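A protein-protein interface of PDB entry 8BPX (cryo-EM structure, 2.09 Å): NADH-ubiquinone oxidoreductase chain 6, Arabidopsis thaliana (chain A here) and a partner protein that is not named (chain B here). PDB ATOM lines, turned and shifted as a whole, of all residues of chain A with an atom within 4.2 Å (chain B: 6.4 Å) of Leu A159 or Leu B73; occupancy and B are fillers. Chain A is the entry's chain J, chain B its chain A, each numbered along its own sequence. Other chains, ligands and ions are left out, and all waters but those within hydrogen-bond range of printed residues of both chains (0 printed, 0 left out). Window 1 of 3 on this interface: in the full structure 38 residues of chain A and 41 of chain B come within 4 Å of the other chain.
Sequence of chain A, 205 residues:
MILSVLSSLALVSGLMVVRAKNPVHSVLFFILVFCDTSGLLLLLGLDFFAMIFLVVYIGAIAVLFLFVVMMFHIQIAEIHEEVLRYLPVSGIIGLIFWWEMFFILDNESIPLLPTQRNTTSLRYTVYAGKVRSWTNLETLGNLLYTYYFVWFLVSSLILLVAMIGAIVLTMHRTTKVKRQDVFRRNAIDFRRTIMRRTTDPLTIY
Of the 9 printed residues of chain A, 4 touch a printed residue of chain B. Hydrophobic or aromatic side chains of chain A within 4 Å of the printed part of chain B: Leu A159 and Met A163. Of the 13 printed residues of chain B, 4 touch a printed residue of chain A. Among the printed residues, 7 pairs touch across the chains. Among the printed residues, no Asp or Glu carboxylate lies within 4 Å of a Lys or Arg side-chain nitrogen of the other chain.
Leu A159 touches just these residues of chain B: Leu B73 (3.7 Å) and Leu B103 (3.98 Å). Printed residues of chain B within 4 Å of Met A163: Ile B70 (3.8 Å) and Leu B103 (3.9 Å). Printed residues of chain A within 4 Å of Ile B70: Met A163 (3.8 Å). Of the printed residues of chain B, Ser A156 touches Phe B99 (3.3 Å) and Leu B103 (3.9 Å). Leu A157 touches none of the printed residues of chain B. Phe B71 touches none of the printed residues of chain A. The nearest residue of chain B that does not touch Leu A159 is Ile B70 (4.1 Å). The nearest printed residue of chain A that does not touch Leu B103 is Leu A160 (4.6 Å).
Ser A155 touches Phe B99. Ser A156 touches Phe B99. Ser A156 touches Leu B103. CD2 of Leu A159 touches CD1 of Leu B73 (3.7 Å). CD2 of Leu B103 touches CB of Leu A159, at 3.98 Å. Ile B70 touches Met A163. Leu B103 touches Met A163 (O to CE, 3.9 Å).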
ATOM      1  N   SER A 155      13.028  -1.609  13.874  1.00  0.00           N
ATOM      2  CA  SER A 155      14.472  -1.581  13.659  1.00  0.00           C
ATOM      3  C   SER A 155      14.898  -0.288  12.966  1.00  0.00           C
ATOM      4  O   SER A 155      15.952   0.286  13.286  1.00  0.00           O
ATOM      5  CB  SER A 155      14.908  -2.798  12.844  1.00  0.00           C
ATOM      6  OG  SER A 155      14.792  -2.546  11.456  1.00  0.00           O
ATOM      7  N   SER A 156      14.096   0.175  12.002  1.00  0.00           N
ATOM      8  CA  SER A 156      14.371   1.481  11.400  1.00  0.00           C
ATOM      9  C   SER A 156      14.389   2.586  12.453  1.00  0.00           C
ATOM     10  O   SER A 156      15.242   3.484  12.413  1.00  0.00           O
ATOM     11  CB  SER A 156      13.341   1.806  10.319  1.00  0.00           C
ATOM     12  OG  SER A 156      12.144   2.310  10.875  1.00  0.00           O
ATOM     13  N   LEU A 157      13.445   2.545  13.393  1.00  0.00           N
ATOM     14  CA  LEU A 157      13.436   3.541  14.465  1.00  0.00           C
ATOM     15  C   LEU A 157      14.717   3.472  15.292  1.00  0.00           C
ATOM     16  O   LEU A 157      15.267   4.506  15.700  1.00  0.00           O
ATOM     17  CB  LEU A 157      12.212   3.349  15.359  1.00  0.00           C
ATOM     18  CG  LEU A 157      10.866   3.819  14.807  1.00  0.00           C
ATOM     19  CD1 LEU A 157       9.780   3.672  15.864  1.00  0.00           C
ATOM     20  CD2 LEU A 157      10.958   5.260  14.318  1.00  0.00           C
ATOM     21  N   ILE A 158      15.200   2.255  15.547  1.00  0.00           N
ATOM     22  CA  ILE A 158      16.446   2.076  16.289  1.00  0.00           C
ATOM     23  C   ILE A 158      17.611   2.739  15.550  1.00  0.00           C
ATOM     24  O   ILE A 158      18.439   3.442  16.151  1.00  0.00           O
ATOM     25  CB  ILE A 158      16.691   0.573  16.536  1.00  0.00           C
ATOM     26  CG1 ILE A 158      15.802   0.061  17.673  1.00  0.00           C
ATOM     27  CG2 ILE A 158      18.149   0.291  16.822  1.00  0.00           C
ATOM     28  CD1 ILE A 158      15.679  -1.448  17.721  1.00  0.00           C
ATOM     29  N   LEU A 159      17.673   2.548  14.232  1.00  0.00           N
ATOM     30  CA  LEU A 159      18.740   3.177  13.453  1.00  0.00           C
ATOM     31  C   LEU A 159      18.628   4.701  13.476  1.00  0.00           C
ATOM     32  O   LEU A 159      19.644   5.406  13.550  1.00  0.00           O
ATOM     33  CB  LEU A 159      18.731   2.653  12.018  1.00  0.00           C
ATOM     34  CG  LEU A 159      19.097   1.173  11.874  1.00  0.00           C
ATOM     35  CD1 LEU A 159      18.999   0.737  10.426  1.00  0.00           C
ATOM     36  CD2 LEU A 159      20.486   0.887  12.443  1.00  0.00           C
ATOM     37  N   LEU A 160      17.400   5.225  13.412  1.00  0.00           N
ATOM     38  CA  LEU A 160      17.209   6.671  13.505  1.00  0.00           C
ATOM     39  C   LEU A 160      17.734   7.209  14.833  1.00  0.00           C
ATOM     40  O   LEU A 160      18.374   8.272  14.877  1.00  0.00           O
ATOM     41  CB  LEU A 160      15.729   7.019  13.331  1.00  0.00           C
ATOM     42  CG  LEU A 160      15.338   8.485  13.546  1.00  0.00           C
ATOM     43  CD1 LEU A 160      16.011   9.364  12.522  1.00  0.00           C
ATOM     44  CD2 LEU A 160      13.828   8.664  13.488  1.00  0.00           C
ATOM     45  N   VAL A 161      17.463   6.489  15.924  1.00  0.00           N
ATOM     46  CA  VAL A 161      18.005   6.880  17.222  1.00  0.00           C
ATOM     47  C   VAL A 161      19.526   6.911  17.170  1.00  0.00           C
ATOM     48  O   VAL A 161      20.158   7.828  17.706  1.00  0.00           O
ATOM     49  CB  VAL A 161      17.500   5.936  18.332  1.00  0.00           C
ATOM     50  CG1 VAL A 161      18.259   6.190  19.629  1.00  0.00           C
ATOM     51  CG2 VAL A 161      16.013   6.121  18.547  1.00  0.00           C
ATOM     52  N   ALA A 162      20.137   5.906  16.538  1.00  0.00           N
ATOM     53  CA  ALA A 162      21.596   5.889  16.436  1.00  0.00           C
ATOM     54  C   ALA A 162      22.116   7.136  15.725  1.00  0.00           C
ATOM     55  O   ALA A 162      23.074   7.769  16.180  1.00  0.00           O
ATOM     56  CB  ALA A 162      22.068   4.626  15.714  1.00  0.00           C
ATOM     57  N   MET A 163      21.484   7.505  14.607  1.00  0.00           N
ATOM     58  CA  MET A 163      21.923   8.684  13.857  1.00  0.00           C
ATOM     59  C   MET A 163      21.815   9.950  14.704  1.00  0.00           C
ATOM     60  O   MET A 163      22.771  10.741  14.806  1.00  0.00           O
ATOM     61  CB  MET A 163      21.096   8.821  12.574  1.00  0.00           C
ATOM     62  CG  MET A 163      20.933   7.515  11.822  1.00  0.00           C
ATOM     63  SD  MET A 163      19.752   7.508  10.459  1.00  0.00           S
ATOM     64  CE  MET A 163      20.449   8.726   9.365  1.00  0.00           C
ATOM     65  N   PHE B  68      28.091   5.530   7.020  1.00  0.00           N
ATOM     66  CA  PHE B  68      28.307   4.334   6.218  1.00  0.00           C
ATOM     67  C   PHE B  68      27.640   3.125   6.848  1.00  0.00           C
ATOM     68  O   PHE B  68      27.091   2.282   6.141  1.00  0.00           O
ATOM     69  CB  PHE B  68      29.794   4.061   6.026  1.00  0.00           C
ATOM     70  CG  PHE B  68      30.064   2.796   5.276  1.00  0.00           C
ATOM     71  CD1 PHE B  68      29.623   2.651   3.972  1.00  0.00           C
ATOM     72  CD2 PHE B  68      30.721   1.738   5.878  1.00  0.00           C
ATOM     73  CE1 PHE B  68      29.854   1.484   3.273  1.00  0.00           C
ATOM     74  CE2 PHE B  68      30.951   0.567   5.184  1.00  0.00           C
ATOM     75  CZ  PHE B  68      30.519   0.440   3.881  1.00  0.00           C
ATOM     76  N   LEU B  69      27.696   3.012   8.176  1.00  0.00           N
ATOM     77  CA  LEU B  69      27.032   1.904   8.855  1.00  0.00           C
ATOM     78  C   LEU B  69      25.534   1.907   8.573  1.00  0.00           C
ATOM     79  O   LEU B  69      24.946   0.872   8.226  1.00  0.00           O
ATOM     80  CB  LEU B  69      27.300   1.992  10.355  1.00  0.00           C
ATOM     81  CG  LEU B  69      26.597   0.986  11.260  1.00  0.00           C
ATOM     82  CD1 LEU B  69      26.973  -0.441  10.894  1.00  0.00           C
ATOM     83  CD2 LEU B  69      26.939   1.296  12.698  1.00  0.00           C
ATOM     84  N   ILE B  70      24.907   3.081   8.699  1.00  0.00           N
ATOM     85  CA  ILE B  70      23.464   3.187   8.482  1.00  0.00           C
ATOM     86  C   ILE B  70      23.106   2.769   7.059  1.00  0.00           C
ATOM     87  O   ILE B  70      22.225   1.926   6.839  1.00  0.00           O
ATOM     88  CB  ILE B  70      22.977   4.616   8.783  1.00  0.00           C
ATOM     89  CG1 ILE B  70      23.277   5.022  10.231  1.00  0.00           C
ATOM     90  CG2 ILE B  70      21.491   4.753   8.466  1.00  0.00           C
ATOM     91  CD1 ILE B  70      23.001   3.960  11.258  1.00  0.00           C
ATOM     92  N   PHE B  71      23.798   3.334   6.068  1.00  0.00           N
ATOM     93  CA  PHE B  71      23.423   3.020   4.692  1.00  0.00           C
ATOM     94  C   PHE B  71      23.868   1.625   4.266  1.00  0.00           C
ATOM     95  O   PHE B  71      23.258   1.036   3.366  1.00  0.00           O
ATOM     96  CB  PHE B  71      23.953   4.090   3.748  1.00  0.00           C
ATOM     97  CG  PHE B  71      23.111   5.328   3.739  1.00  0.00           C
ATOM     98  CD1 PHE B  71      23.314   6.330   4.673  1.00  0.00           C
ATOM     99  CD2 PHE B  71      22.075   5.466   2.831  1.00  0.00           C
ATOM    100  CE1 PHE B  71      22.525   7.465   4.677  1.00  0.00           C
ATOM    101  CE2 PHE B  71      21.283   6.594   2.829  1.00  0.00           C
ATOM    102  CZ  PHE B  71      21.508   7.597   3.753  1.00  0.00           C
ATOM    103  N   ASP B  72      24.885   1.070   4.925  1.00  0.00           N
ATOM    104  CA  ASP B  72      25.233  -0.333   4.758  1.00  0.00           C
ATOM    105  C   ASP B  72      24.073  -1.227   5.168  1.00  0.00           C
ATOM    106  O   ASP B  72      23.704  -2.160   4.444  1.00  0.00           O
ATOM    107  CB  ASP B  72      26.476  -0.636   5.596  1.00  0.00           C
ATOM    108  CG  ASP B  72      27.287  -1.778   5.053  1.00  0.00           C
ATOM    109  OD1 ASP B  72      27.770  -1.678   3.908  1.00  0.00           O
ATOM    110  OD2 ASP B  72      27.455  -2.774   5.786  1.00  0.00           O
ATOM    111  N   LEU B  73      23.470  -0.943   6.328  1.00  0.00           N
ATOM    112  CA  LEU B  73      22.295  -1.714   6.723  1.00  0.00           C
ATOM    113  C   LEU B  73      21.122  -1.473   5.781  1.00  0.00           C
ATOM    114  O   LEU B  73      20.318  -2.385   5.551  1.00  0.00           O
ATOM    115  CB  LEU B  73      21.885  -1.399   8.159  1.00  0.00           C
ATOM    116  CG  LEU B  73      22.778  -2.016   9.229  1.00  0.00           C
ATOM    117  CD1 LEU B  73      22.862  -1.088  10.421  1.00  0.00           C
ATOM    118  CD2 LEU B  73      22.309  -3.410   9.622  1.00  0.00           C
ATOM    119  N   GLU B  74      21.002  -0.260   5.237  1.00  0.00           N
ATOM    120  CA  GLU B  74      19.952   0.000   4.253  1.00  0.00           C
ATOM    121  C   GLU B  74      20.106  -0.901   3.028  1.00  0.00           C
ATOM    122  O   GLU B  74      19.132  -1.501   2.559  1.00  0.00           O
ATOM    123  CB  GLU B  74      19.962   1.470   3.838  1.00  0.00           C
ATOM    124  CG  GLU B  74      18.606   1.990   3.400  1.00  0.00           C
ATOM    125  CD  GLU B  74      18.597   3.488   3.164  1.00  0.00           C
ATOM    126  OE1 GLU B  74      18.082   4.225   4.027  1.00  0.00           O
ATOM    127  OE2 GLU B  74      19.101   3.927   2.109  1.00  0.00           O
ATOM    128  N   VAL B  75      21.328  -1.013   2.501  1.00  0.00           N
ATOM    129  CA  VAL B  75      21.570  -1.903   1.364  1.00  0.00           C
ATOM    130  C   VAL B  75      21.291  -3.357   1.752  1.00  0.00           C
ATOM    131  O   VAL B  75      20.690  -4.130   0.979  1.00  0.00           O
ATOM    132  CB  VAL B  75      23.011  -1.720   0.846  1.00  0.00           C
ATOM    133  CG1 VAL B  75      23.334  -2.746  -0.222  1.00  0.00           C
ATOM    134  CG2 VAL B  75      23.214  -0.305   0.311  1.00  0.00           C
ATOM    135  N   THR B  76      21.739  -3.750   2.948  1.00  0.00           N
ATOM    136  CA  THR B  76      21.468  -5.086   3.466  1.00  0.00           C
ATOM    137  C   THR B  76      19.980  -5.409   3.408  1.00  0.00           C
ATOM    138  O   THR B  76      19.578  -6.453   2.886  1.00  0.00           O
ATOM    139  CB  THR B  76      21.986  -5.196   4.903  1.00  0.00           C
ATOM    140  OG1 THR B  76      23.416  -5.124   4.910  1.00  0.00           O
ATOM    141  CG2 THR B  76      21.527  -6.501   5.551  1.00  0.00           C
ATOM    142  N   PHE B  77      19.146  -4.505   3.923  1.00  0.00           N
ATOM    143  CA  PHE B  77      17.705  -4.728   3.906  1.00  0.00           C
ATOM    144  C   PHE B  77      17.114  -4.603   2.507  1.00  0.00           C
ATOM    145  O   PHE B  77      16.046  -5.163   2.250  1.00  0.00           O
ATOM    146  CB  PHE B  77      17.015  -3.760   4.865  1.00  0.00           C
ATOM    147  CG  PHE B  77      16.975  -4.247   6.285  1.00  0.00           C
ATOM    148  CD1 PHE B  77      16.117  -5.268   6.655  1.00  0.00           C
ATOM    149  CD2 PHE B  77      17.800  -3.691   7.247  1.00  0.00           C
ATOM    150  CE1 PHE B  77      16.078  -5.721   7.959  1.00  0.00           C
ATOM    151  CE2 PHE B  77      17.766  -4.141   8.556  1.00  0.00           C
ATOM    152  CZ  PHE B  77      16.903  -5.157   8.910  1.00  0.00           C
ATOM    153  N   PHE B  78      17.782  -3.885   1.602  1.00  0.00           N
ATOM    154  CA  PHE B  78      17.303  -3.783   0.227  1.00  0.00           C
ATOM    155  C   PHE B  78      17.414  -5.114  -0.512  1.00  0.00           C
ATOM    156  O   PHE B  78      16.566  -5.428  -1.354  1.00  0.00           O
ATOM    157  CB  PHE B  78      18.081  -2.706  -0.527  1.00  0.00           C
ATOM    158  CG  PHE B  78      17.376  -1.379  -0.609  1.00  0.00           C
ATOM    159  CD1 PHE B  78      16.053  -1.301  -1.019  1.00  0.00           C
ATOM    160  CD2 PHE B  78      18.047  -0.206  -0.300  1.00  0.00           C
ATOM    161  CE1 PHE B  78      15.407  -0.081  -1.103  1.00  0.00           C
ATOM    162  CE2 PHE B  78      17.409   1.019  -0.382  1.00  0.00           C
ATOM    163  CZ  PHE B  78      16.089   1.081  -0.786  1.00  0.00           C
ATOM    164  N   PHE B  99      10.115   2.349   5.791  1.00  0.00           N
ATOM    165  CA  PHE B  99      11.480   2.183   6.289  1.00  0.00           C
ATOM    166  C   PHE B  99      12.393   3.285   5.755  1.00  0.00           C
ATOM    167  O   PHE B  99      13.096   3.972   6.517  1.00  0.00           O
ATOM    168  CB  PHE B  99      11.991   0.802   5.872  1.00  0.00           C
ATOM    169  CG  PHE B  99      13.335   0.433   6.437  1.00  0.00           C
ATOM    170  CD1 PHE B  99      13.442  -0.166   7.678  1.00  0.00           C
ATOM    171  CD2 PHE B  99      14.488   0.641   5.698  1.00  0.00           C
ATOM    172  CE1 PHE B  99      14.678  -0.527   8.189  1.00  0.00           C
ATOM    173  CE2 PHE B  99      15.725   0.281   6.200  1.00  0.00           C
ATOM    174  CZ  PHE B  99      15.822  -0.297   7.450  1.00  0.00           C
ATOM    175  N   LEU B 103      14.511   6.457   7.586  1.00  0.00           N
ATOM    176  CA  LEU B 103      15.955   6.626   7.429  1.00  0.00           C
ATOM    177  C   LEU B 103      16.295   7.939   6.721  1.00  0.00           C
ATOM    178  O   LEU B 103      17.306   8.577   7.029  1.00  0.00           O
ATOM    179  CB  LEU B 103      16.548   5.427   6.687  1.00  0.00           C
ATOM    180  CG  LEU B 103      16.557   4.119   7.490  1.00  0.00           C
ATOM    181  CD1 LEU B 103      17.545   3.118   6.912  1.00  0.00           C
ATOM    182  CD2 LEU B 103      16.845   4.369   8.963  1.00  0.00           C
